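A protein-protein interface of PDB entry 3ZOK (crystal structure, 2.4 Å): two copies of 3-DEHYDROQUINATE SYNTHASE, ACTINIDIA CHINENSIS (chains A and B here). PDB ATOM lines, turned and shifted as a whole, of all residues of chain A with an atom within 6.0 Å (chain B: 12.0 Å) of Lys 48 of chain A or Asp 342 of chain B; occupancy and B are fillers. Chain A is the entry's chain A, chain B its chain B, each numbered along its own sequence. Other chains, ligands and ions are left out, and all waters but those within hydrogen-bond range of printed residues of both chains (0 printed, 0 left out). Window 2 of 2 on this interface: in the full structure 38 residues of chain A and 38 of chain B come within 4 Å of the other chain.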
ATOM      1  N   VAL A  45      13.719  16.956 -20.853  1.00  0.00           N
ATOM      2  CA  VAL A  45      13.723  16.078 -19.706  1.00  0.00           C
ATOM      3  C   VAL A  45      15.049  16.296 -18.983  1.00  0.00           C
ATOM      4  O   VAL A  45      16.065  15.783 -19.414  1.00  0.00           O
ATOM      5  CB  VAL A  45      13.547  14.620 -20.184  1.00  0.00           C
ATOM      6  CG1 VAL A  45      13.766  13.623 -19.052  1.00  0.00           C
ATOM      7  CG2 VAL A  45      12.159  14.457 -20.791  1.00  0.00           C
ATOM      8  N   HIS A  46      15.027  17.085 -17.917  1.00  0.00           N
ATOM      9  CA  HIS A  46      16.228  17.466 -17.171  1.00  0.00           C
ATOM     10  C   HIS A  46      16.456  16.628 -15.881  1.00  0.00           C
ATOM     11  O   HIS A  46      17.146  17.043 -14.963  1.00  0.00           O
ATOM     12  CB  HIS A  46      16.185  18.971 -16.836  1.00  0.00           C
ATOM     13  CG  HIS A  46      15.881  19.848 -18.022  1.00  0.00           C
ATOM     14  ND1 HIS A  46      15.528  21.175 -17.899  1.00  0.00           N
ATOM     15  CD2 HIS A  46      15.851  19.579 -19.352  1.00  0.00           C
ATOM     16  CE1 HIS A  46      15.298  21.685 -19.095  1.00  0.00           C
ATOM     17  NE2 HIS A  46      15.488  20.737 -19.994  1.00  0.00           N
ATOM     18  N   GLY A  47      15.880  15.436 -15.833  1.00  0.00           N
ATOM     19  CA  GLY A  47      16.062  14.542 -14.715  1.00  0.00           C
ATOM     20  C   GLY A  47      16.036  13.111 -15.202  1.00  0.00           C
ATOM     21  O   GLY A  47      15.861  12.848 -16.400  1.00  0.00           O
ATOM     22  N   LYS A  48      16.198  12.184 -14.268  1.00  0.00           N
ATOM     23  CA  LYS A  48      16.348  10.778 -14.611  1.00  0.00           C
ATOM     24  C   LYS A  48      15.029  10.072 -14.862  1.00  0.00           C
ATOM     25  O   LYS A  48      15.010   9.036 -15.520  1.00  0.00           O
ATOM     26  CB  LYS A  48      17.093  10.052 -13.487  1.00  0.00           C
ATOM     27  CG  LYS A  48      18.591   9.978 -13.698  1.00  0.00           C
ATOM     28  CD  LYS A  48      19.275   9.457 -12.447  1.00  0.00           C
ATOM     29  CE  LYS A  48      20.561   8.706 -12.787  1.00  0.00           C
ATOM     30  NZ  LYS A  48      21.330   8.283 -11.572  1.00  0.00           N
ATOM     31  N   ARG A  49      13.944  10.624 -14.323  1.00  0.00           N
ATOM     32  CA  ARG A  49      12.686   9.903 -14.182  1.00  0.00           C
ATOM     33  C   ARG A  49      11.546  10.692 -14.764  1.00  0.00           C
ATOM     34  O   ARG A  49      11.535  11.917 -14.732  1.00  0.00           O
ATOM     35  CB  ARG A  49      12.406   9.578 -12.711  1.00  0.00           C
ATOM     36  CG  ARG A  49      13.461   8.644 -12.123  1.00  0.00           C
ATOM     37  CD  ARG A  49      13.145   8.217 -10.713  1.00  0.00           C
ATOM     38  NE  ARG A  49      12.129   7.171 -10.697  1.00  0.00           N
ATOM     39  CZ  ARG A  49      11.366   6.888  -9.655  1.00  0.00           C
ATOM     40  NH1 ARG A  49      11.483   7.572  -8.548  1.00  0.00           N
ATOM     41  NH2 ARG A  49      10.444   5.937  -9.732  1.00  0.00           N
ATOM     42  N   VAL A  50      10.582   9.965 -15.305  1.00  0.00           N
ATOM     43  CA  VAL A  50       9.507  10.564 -16.046  1.00  0.00           C
ATOM     44  C   VAL A  50       8.211   9.854 -15.680  1.00  0.00           C
ATOM     45  O   VAL A  50       8.210   8.661 -15.437  1.00  0.00           O
ATOM     46  CB  VAL A  50       9.817  10.470 -17.544  1.00  0.00           C
ATOM     47  CG1 VAL A  50       8.597  10.772 -18.405  1.00  0.00           C
ATOM     48  CG2 VAL A  50      10.964  11.419 -17.870  1.00  0.00           C
ATOM     49  N   ASN A  76      19.522   6.444 -19.538  1.00  0.00           N
ATOM     50  CA  ASN A  76      19.538   6.926 -18.156  1.00  0.00           C
ATOM     51  C   ASN A  76      18.215   7.554 -17.725  1.00  0.00           C
ATOM     52  O   ASN A  76      18.094   8.066 -16.608  1.00  0.00           O
ATOM     53  CB  ASN A  76      20.729   7.844 -17.913  1.00  0.00           C
ATOM     54  CG  ASN A  76      20.791   8.964 -18.903  1.00  0.00           C
ATOM     55  OD1 ASN A  76      20.500   8.784 -20.087  1.00  0.00           O
ATOM     56  ND2 ASN A  76      21.134  10.139 -18.429  1.00  0.00           N
ATOM     57  N   VAL A  77      17.231   7.463 -18.622  1.00  0.00           N
ATOM     58  CA  VAL A  77      15.874   7.907 -18.409  1.00  0.00           C
ATOM     59  C   VAL A  77      14.993   6.661 -18.185  1.00  0.00           C
ATOM     60  O   VAL A  77      15.068   5.709 -18.953  1.00  0.00           O
ATOM     61  CB  VAL A  77      15.397   8.740 -19.634  1.00  0.00           C
ATOM     62  CG1 VAL A  77      13.887   8.661 -19.852  1.00  0.00           C
ATOM     63  CG2 VAL A  77      15.842  10.190 -19.489  1.00  0.00           C
ATOM     64  N   SER A  78      14.194   6.671 -17.114  1.00  0.00           N
ATOM     65  CA  SER A  78      13.222   5.616 -16.843  1.00  0.00           C
ATOM     66  C   SER A  78      11.854   6.259 -16.730  1.00  0.00           C
ATOM     67  O   SER A  78      11.717   7.356 -16.192  1.00  0.00           O
ATOM     68  CB  SER A  78      13.557   4.868 -15.556  1.00  0.00           C
ATOM     69  OG  SER A  78      13.542   5.750 -14.453  1.00  0.00           O
ATOM     70  N   VAL A  79      10.854   5.552 -17.244  1.00  0.00           N
ATOM     71  CA  VAL A  79       9.527   6.084 -17.498  1.00  0.00           C
ATOM     72  C   VAL A  79       8.482   5.252 -16.748  1.00  0.00           C
ATOM     73  O   VAL A  79       8.511   4.022 -16.782  1.00  0.00           O
ATOM     74  CB  VAL A  79       9.228   6.051 -19.016  1.00  0.00           C
ATOM     75  CG1 VAL A  79       7.764   6.329 -19.310  1.00  0.00           C
ATOM     76  CG2 VAL A  79      10.090   7.060 -19.736  1.00  0.00           C
ATOM     77  N   ASP A 109      10.613  12.779  -7.465  1.00  0.00           N
ATOM     78  CA  ASP A 109      11.150  13.898  -6.712  1.00  0.00           C
ATOM     79  C   ASP A 109      11.113  15.128  -7.634  1.00  0.00           C
ATOM     80  O   ASP A 109      10.590  15.029  -8.772  1.00  0.00           O
ATOM     81  CB  ASP A 109      12.556  13.568  -6.182  1.00  0.00           C
ATOM     82  CG  ASP A 109      13.574  13.254  -7.291  1.00  0.00           C
ATOM     83  OD1 ASP A 109      13.752  14.058  -8.245  1.00  0.00           O
ATOM     84  OD2 ASP A 109      14.223  12.184  -7.207  1.00  0.00           O
ATOM     85  N   ARG A 111      13.101  16.540  -9.568  1.00  0.00           N
ATOM     86  CA  ARG A 111      13.772  16.442 -10.826  1.00  0.00           C
ATOM     87  C   ARG A 111      12.987  15.626 -11.823  1.00  0.00           C
ATOM     88  O   ARG A 111      13.451  15.460 -12.928  1.00  0.00           O
ATOM     89  CB  ARG A 111      15.135  15.779 -10.649  1.00  0.00           C
ATOM     90  CG  ARG A 111      16.058  16.461  -9.661  1.00  0.00           C
ATOM     91  CD  ARG A 111      16.277  17.916 -10.003  1.00  0.00           C
ATOM     92  NE  ARG A 111      17.401  18.455  -9.248  1.00  0.00           N
ATOM     93  CZ  ARG A 111      17.573  19.738  -8.945  1.00  0.00           C
ATOM     94  NH1 ARG A 111      16.695  20.670  -9.331  1.00  0.00           N
ATOM     95  NH2 ARG A 111      18.638  20.087  -8.237  1.00  0.00           N
ATOM     96  N   CYS A 112      11.849  15.058 -11.438  1.00  0.00           N
ATOM     97  CA  CYS A 112      11.072  14.245 -12.372  1.00  0.00           C
ATOM     98  C   CYS A 112      10.337  15.163 -13.316  1.00  0.00           C
ATOM     99  O   CYS A 112      10.278  16.353 -13.075  1.00  0.00           O
ATOM    100  CB  CYS A 112      10.049  13.375 -11.636  1.00  0.00           C
ATOM    101  SG  CYS A 112       8.654  14.341 -10.991  1.00  0.00           S
ATOM    102  N   SER B 252      15.722  27.120  -5.382  1.00  0.00           N
ATOM    103  CA  SER B 252      16.818  26.641  -6.202  1.00  0.00           C
ATOM    104  C   SER B 252      17.986  26.124  -5.361  1.00  0.00           C
ATOM    105  O   SER B 252      18.578  25.107  -5.667  1.00  0.00           O
ATOM    106  CB  SER B 252      17.315  27.755  -7.112  1.00  0.00           C
ATOM    107  OG  SER B 252      16.657  27.697  -8.355  1.00  0.00           O
ATOM    108  N   MET B 334      11.931   9.708   4.803  1.00  0.00           N
ATOM    109  CA  MET B 334      12.945  10.647   4.333  1.00  0.00           C
ATOM    110  C   MET B 334      13.136  10.542   2.832  1.00  0.00           C
ATOM    111  O   MET B 334      13.446  11.529   2.164  1.00  0.00           O
ATOM    112  CB  MET B 334      14.266  10.419   5.074  1.00  0.00           C
ATOM    113  CG  MET B 334      14.243  11.010   6.465  1.00  0.00           C
ATOM    114  SD  MET B 334      15.558  10.404   7.528  1.00  0.00           S
ATOM    115  CE  MET B 334      16.885  11.573   7.225  1.00  0.00           C
ATOM    116  N   ALA B 335      12.909   9.350   2.306  1.00  0.00           N
ATOM    117  CA  ALA B 335      12.944   9.083   0.874  1.00  0.00           C
ATOM    118  C   ALA B 335      11.984   9.941   0.041  1.00  0.00           C
ATOM    119  O   ALA B 335      12.125   9.986  -1.178  1.00  0.00           O
ATOM    120  CB  ALA B 335      12.678   7.595   0.624  1.00  0.00           C
ATOM    121  N   VAL B 336      11.010  10.593   0.670  1.00  0.00           N
ATOM    122  CA  VAL B 336      10.104  11.481  -0.054  1.00  0.00           C
ATOM    123  C   VAL B 336      10.255  12.914   0.449  1.00  0.00           C
ATOM    124  O   VAL B 336       9.404  13.798   0.197  1.00  0.00           O
ATOM    125  CB  VAL B 336       8.641  10.997   0.002  1.00  0.00           C
ATOM    126  CG1 VAL B 336       8.513   9.643  -0.671  1.00  0.00           C
ATOM    127  CG2 VAL B 336       8.119  10.909   1.427  1.00  0.00           C
ATOM    128  N   ASP B 337      11.360  13.168   1.146  1.00  0.00           N
ATOM    129  CA  ASP B 337      11.692  14.544   1.421  1.00  0.00           C
ATOM    130  C   ASP B 337      11.863  15.307   0.092  1.00  0.00           C
ATOM    131  O   ASP B 337      12.315  14.735  -0.901  1.00  0.00           O
ATOM    132  CB  ASP B 337      12.953  14.651   2.263  1.00  0.00           C
ATOM    133  CG  ASP B 337      13.166  16.028   2.747  1.00  0.00           C
ATOM    134  OD1 ASP B 337      13.576  16.873   1.914  1.00  0.00           O
ATOM    135  OD2 ASP B 337      12.860  16.272   3.933  1.00  0.00           O
ATOM    136  N   LYS B 338      11.523  16.582   0.088  1.00  0.00           N
ATOM    137  CA  LYS B 338      11.595  17.399  -1.106  1.00  0.00           C
ATOM    138  C   LYS B 338      13.022  17.829  -1.413  1.00  0.00           C
ATOM    139  O   LYS B 338      13.283  18.448  -2.427  1.00  0.00           O
ATOM    140  CB  LYS B 338      10.629  18.582  -1.018  1.00  0.00           C
ATOM    141  CG  LYS B 338       9.169  18.158  -1.058  1.00  0.00           C
ATOM    142  CD  LYS B 338       8.196  19.319  -1.020  1.00  0.00           C
ATOM    143  CE  LYS B 338       8.211  20.036   0.310  1.00  0.00           C
ATOM    144  NZ  LYS B 338       7.783  19.204   1.458  1.00  0.00           N
ATOM    145  N   LYS B 339      13.935  17.515  -0.502  1.00  0.00           N
ATOM    146  CA  LYS B 339      15.349  17.794  -0.682  1.00  0.00           C
ATOM    147  C   LYS B 339      16.030  16.665  -1.451  1.00  0.00           C
ATOM    148  O   LYS B 339      17.216  16.725  -1.754  1.00  0.00           O
ATOM    149  CB  LYS B 339      16.028  18.033   0.657  1.00  0.00           C
ATOM    150  CG  LYS B 339      15.721  19.386   1.272  1.00  0.00           C
ATOM    151  CD  LYS B 339      16.135  19.443   2.727  1.00  0.00           C
ATOM    152  CE  LYS B 339      14.954  19.273   3.660  1.00  0.00           C
ATOM    153  NZ  LYS B 339      15.341  18.768   5.005  1.00  0.00           N
ATOM    154  N   VAL B 340      15.264  15.630  -1.759  1.00  0.00           N
ATOM    155  CA  VAL B 340      15.753  14.566  -2.609  1.00  0.00           C
ATOM    156  C   VAL B 340      15.761  15.011  -4.073  1.00  0.00           C
ATOM    157  O   VAL B 340      14.777  15.533  -4.579  1.00  0.00           O
ATOM    158  CB  VAL B 340      14.906  13.289  -2.453  1.00  0.00           C
ATOM    159  CG1 VAL B 340      15.287  12.256  -3.492  1.00  0.00           C
ATOM    160  CG2 VAL B 340      15.046  12.723  -1.056  1.00  0.00           C
ATOM    161  N   ALA B 341      16.877  14.783  -4.750  1.00  0.00           N
ATOM    162  CA  ALA B 341      17.001  15.145  -6.161  1.00  0.00           C
ATOM    163  C   ALA B 341      17.650  13.983  -6.939  1.00  0.00           C
ATOM    164  O   ALA B 341      18.729  13.512  -6.574  1.00  0.00           O
ATOM    165  CB  ALA B 341      17.809  16.418  -6.300  1.00  0.00           C
ATOM    166  N   ASP B 342      16.972  13.526  -7.994  1.00  0.00           N
ATOM    167  CA  ASP B 342      17.342  12.316  -8.735  1.00  0.00           C
ATOM    168  C   ASP B 342      17.750  11.151  -7.823  1.00  0.00           C
ATOM    169  O   ASP B 342      18.746  10.469  -8.064  1.00  0.00           O
ATOM    170  CB  ASP B 342      18.411  12.629  -9.796  1.00  0.00           C
ATOM    171  CG  ASP B 342      17.834  13.373 -11.031  1.00  0.00           C
ATOM    172  OD1 ASP B 342      16.776  12.970 -11.571  1.00  0.00           O
ATOM    173  OD2 ASP B 342      18.461  14.356 -11.465  1.00  0.00           O
ATOM    174  N   GLY B 343      16.938  10.924  -6.787  1.00  0.00           N
ATOM    175  CA  GLY B 343      17.085   9.768  -5.902  1.00  0.00           C
ATOM    176  C   GLY B 343      18.109   9.978  -4.799  1.00  0.00           C
ATOM    177  O   GLY B 343      18.386   9.079  -4.008  1.00  0.00           O
ATOM    178  N   LEU B 344      18.669  11.172  -4.741  1.00  0.00           N
ATOM    179  CA  LEU B 344      19.688  11.492  -3.765  1.00  0.00           C
ATOM    180  C   LEU B 344      19.122  12.383  -2.672  1.00  0.00           C
ATOM    181  O   LEU B 344      18.646  13.470  -2.950  1.00  0.00           O
ATOM    182  CB  LEU B 344      20.817  12.241  -4.467  1.00  0.00           C
ATOM    183  CG  LEU B 344      22.089  12.522  -3.705  1.00  0.00           C
ATOM    184  CD1 LEU B 344      22.683  11.228  -3.165  1.00  0.00           C
ATOM    185  CD2 LEU B 344      23.060  13.228  -4.637  1.00  0.00           C
ATOM    186  N   LEU B 345      19.232  11.946  -1.425  1.00  0.00           N
ATOM    187  CA  LEU B 345      18.738  12.715  -0.306  1.00  0.00           C
ATOM    188  C   LEU B 345      19.766  13.734   0.156  1.00  0.00           C
ATOM    189  O   LEU B 345      20.815  13.361   0.703  1.00  0.00           O
ATOM    190  CB  LEU B 345      18.374  11.792   0.857  1.00  0.00           C
ATOM    191  CG  LEU B 345      17.997  12.478   2.174  1.00  0.00           C
ATOM    192  CD1 LEU B 345      16.861  13.480   2.002  1.00  0.00           C
ATOM    193  CD2 LEU B 345      17.656  11.442   3.238  1.00  0.00           C
ATOM    194  N   ARG B 346      19.446  15.016  -0.014  1.00  0.00           N
ATOM    195  CA  ARG B 346      20.319  16.079   0.444  1.00  0.00           C
ATOM    196  C   ARG B 346      19.796  16.651   1.730  1.00  0.00           C
ATOM    197  O   ARG B 346      18.599  16.819   1.900  1.00  0.00           O
ATOM    198  CB  ARG B 346      20.433  17.150  -0.621  1.00  0.00           C
ATOM    199  CG  ARG B 346      20.891  16.574  -1.945  1.00  0.00           C
ATOM    200  CD  ARG B 346      21.573  17.604  -2.817  1.00  0.00           C
ATOM    201  NE  ARG B 346      20.719  18.045  -3.907  1.00  0.00           N
ATOM    202  CZ  ARG B 346      20.937  19.143  -4.622  1.00  0.00           C
ATOM    203  NH1 ARG B 346      21.971  19.940  -4.358  1.00  0.00           N
ATOM    204  NH2 ARG B 346      20.104  19.458  -5.604  1.00  0.00           N
ATOM    205  N   LEU B 347      20.705  16.944   2.639  1.00  0.00           N
ATOM    206  CA  LEU B 347      20.340  17.310   4.001  1.00  0.00           C
ATOM    207  C   LEU B 347      20.881  18.680   4.372  1.00  0.00           C
ATOM    208  O   LEU B 347      21.784  19.184   3.736  1.00  0.00           O
ATOM    209  CB  LEU B 347      20.880  16.278   4.993  1.00  0.00           C
ATOM    210  CG  LEU B 347      20.416  14.818   4.831  1.00  0.00           C
ATOM    211  CD1 LEU B 347      21.328  13.898   5.631  1.00  0.00           C
ATOM    212  CD2 LEU B 347      18.968  14.606   5.254  1.00  0.00           C
ATOM    213  N   PHE B 359      23.936  22.700   2.685  1.00  0.00           N
ATOM    214  CA  PHE B 359      22.933  21.837   2.103  1.00  0.00           C
ATOM    215  C   PHE B 359      23.732  20.947   1.169  1.00  0.00           C
ATOM    216  O   PHE B 359      24.288  21.425   0.185  1.00  0.00           O
ATOM    217  CB  PHE B 359      21.943  22.701   1.320  1.00  0.00           C
ATOM    218  CG  PHE B 359      20.900  21.927   0.572  1.00  0.00           C
ATOM    219  CD1 PHE B 359      20.358  20.770   1.100  1.00  0.00           C
ATOM    220  CD2 PHE B 359      20.451  22.371  -0.658  1.00  0.00           C
ATOM    221  CE1 PHE B 359      19.396  20.066   0.408  1.00  0.00           C
ATOM    222  CE2 PHE B 359      19.489  21.672  -1.356  1.00  0.00           C
ATOM    223  CZ  PHE B 359      18.960  20.517  -0.821  1.00  0.00           C
ATOM    224  N   THR B 360      23.798  19.655   1.471  1.00  0.00           N
ATOM    225  CA  THR B 360      24.685  18.770   0.727  1.00  0.00           C
ATOM    226  C   THR B 360      24.142  17.382   0.444  1.00  0.00           C
ATOM    227  O   THR B 360      23.422  16.800   1.250  1.00  0.00           O
ATOM    228  CB  THR B 360      26.031  18.589   1.458  1.00  0.00           C
ATOM    229  OG1 THR B 360      25.802  18.043   2.760  1.00  0.00           O
ATOM    230  CG2 THR B 360      26.754  19.914   1.581  1.00  0.00           C
ATOM    231  N   GLY B 361      24.521  16.850  -0.711  1.00  0.00           N
ATOM    232  CA  GLY B 361      24.334  15.450  -1.012  1.00  0.00           C
ATOM    233  C   GLY B 361      25.564  14.662  -0.610  1.00  0.00           C
ATOM    234  O   GLY B 361      25.563  13.434  -0.652  1.00  0.00           O
ATOM    235  N   ASP B 362      26.623  15.364  -0.214  1.00  0.00           N
ATOM    236  CA  ASP B 362      27.859  14.680   0.145  1.00  0.00           C
ATOM    237  C   ASP B 362      28.019  14.565   1.648  1.00  0.00           C
ATOM    238  O   ASP B 362      28.386  15.520   2.324  1.00  0.00           O
ATOM    239  CB  ASP B 362      29.072  15.418  -0.423  1.00  0.00           C
ATOM    240  CG  ASP B 362      28.872  15.856  -1.853  1.00  0.00           C
ATOM    241  OD1 ASP B 362      28.018  15.269  -2.543  1.00  0.00           O
ATOM    242  OD2 ASP B 362      29.573  16.791  -2.288  1.00  0.00           O
ATOM    243  N   TYR B 363      27.772  13.368   2.158  1.00  0.00           N
ATOM    244  CA  TYR B 363      28.028  13.054   3.549  1.00  0.00           C
ATOM    245  C   TYR B 363      28.206  11.555   3.654  1.00  0.00           C
ATOM    246  O   TYR B 363      27.735  10.810   2.797  1.00  0.00           O
ATOM    247  CB  TYR B 363      26.880  13.528   4.446  1.00  0.00           C
ATOM    248  CG  TYR B 363      25.507  13.128   3.959  1.00  0.00           C
ATOM    249  CD1 TYR B 363      24.977  11.883   4.263  1.00  0.00           C
ATOM    250  CD2 TYR B 363      24.739  13.998   3.200  1.00  0.00           C
ATOM    251  CE1 TYR B 363      23.721  11.515   3.823  1.00  0.00           C
ATOM    252  CE2 TYR B 363      23.483  13.640   2.755  1.00  0.00           C
ATOM    253  CZ  TYR B 363      22.979  12.397   3.070  1.00  0.00           C
ATOM    254  OH  TYR B 363      21.730  12.036   2.627  1.00  0.00           O
ATOM    255  N   ARG B 365      27.112   8.227   4.791  1.00  0.00           N
ATOM    256  CA  ARG B 365      25.861   7.598   5.207  1.00  0.00           C
ATOM    257  C   ARG B 365      25.954   6.862   6.541  1.00  0.00           C
ATOM    258  O   ARG B 365      24.939   6.672   7.190  1.00  0.00           O
ATOM    259  CB  ARG B 365      25.350   6.654   4.117  1.00  0.00           C
ATOM    260  CG  ARG B 365      24.427   7.328   3.109  1.00  0.00           C
ATOM    261  CD  ARG B 365      25.029   8.609   2.550  1.00  0.00           C
ATOM    262  NE  ARG B 365      24.207   9.268   1.531  1.00  0.00           N
ATOM    263  CZ  ARG B 365      24.579  10.349   0.842  1.00  0.00           C
ATOM    264  NH1 ARG B 365      25.757  10.915   1.056  1.00  0.00           N
ATOM    265  NH2 ARG B 365      23.769  10.871  -0.077  1.00  0.00           N
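Lys 48 of chain A touches just one residue of chain B: Asp 342.
Of the printed residues of chain A, Asp 342 of chain B touches Gly 47 (3.6 Å), Lys 48 (2.9 Å), Asp 109 (3.2 Å) and Arg 111 (3.4 Å).
No residue of chain B comes within 4 Å of Val 50 of chain A.
Asp 109 of chain A touches just these residues of chain B: Val 340 (3.4 Å), Ala 341 (3.9 Å), Asp 342 (3.2 Å) and Gly 343 (3.0 Å).
Arg 111 of chain A touches three residues of chain B.
Printed residues of chain A within 4 Å of Ala 341 of chain B: Asp 109 and Arg 111.
Of the printed residues of chain A, Gly 343 of chain B touches Asp 109 (3.0 Å).
Printed residues of chain A within 4 Å of Val 340 of chain B: Asp 109.
Of the printed residues of chain A, Arg 346 of chain B touches Arg 111.
Ala 335 of chain B touches none of the printed residues of chain A.
Asp 337 of chain B touches none of the printed residues of chain A.
The nearest printed residue of chain A that does not touch Asp 342 of chain B is Arg 49 of chain A (4.6 Å).
Printed residues of chain A that touch a printed residue of chain B: Gly 47, Lys 48, Asp 109 and Arg 111.
Among the printed residues, no Asp or Glu carboxylate lies within 4 Å of a Lys or Arg side-chain nitrogen of the other chain.
No position is printed for both chains.
Of the 9 pairs that touch across the chains among the printed residues, none has its exchanged pair printed and touching as well.
Among the printed residues, pairs that only touch across the chains: Gly 47 of chain A with Asp 342 of chain B (3.6 Å), Asp 109 of chain A with Val 340 of chain B (3.4 Å), Asp 109 of chain A with Ala 341 of chain B (3.9 Å), Arg 111 of chain A with Ala 341 of chain B (3.6 Å) and Arg 111 of chain A with Asp 342 of chain B (3.4 Å).
N of Ser 78 of chain A lies within hydrogen-bond range of O of Lys 48 of chain A.
OD1 of Asp 109 of chain A sits at hydrogen-bond distance from N of Arg 111 of chain A.
The backbone carbonyl oxygen (O) of Asp 109 of chain A is in hydrogen-bond range of the side-chain sulfur (SG) of Cys 112 of chain A (3.0 Å).
O of Lys 339 of chain B is in hydrogen-bond range of N of Arg 346 of chain B (3.3 Å).
N of Lys 48 of chain A sits at hydrogen-bond distance from OD1 of Asp 342 of chain B (2.9 Å).
OD2 of Asp 109 of chain A is in hydrogen-bond range of N of Asp 342 of chain B (3.2 Å).
The backbone NH (N) of Gly 343 of chain B sits at hydrogen-bond distance from the side-chain carboxylate (OD2) of Asp 109 of chain A (3.0 Å).
The guanidinium group (NH2) of Arg 111 of chain A lies close to the guanidinium group (NH2) of Arg 346 of chain B (3.1 Å).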
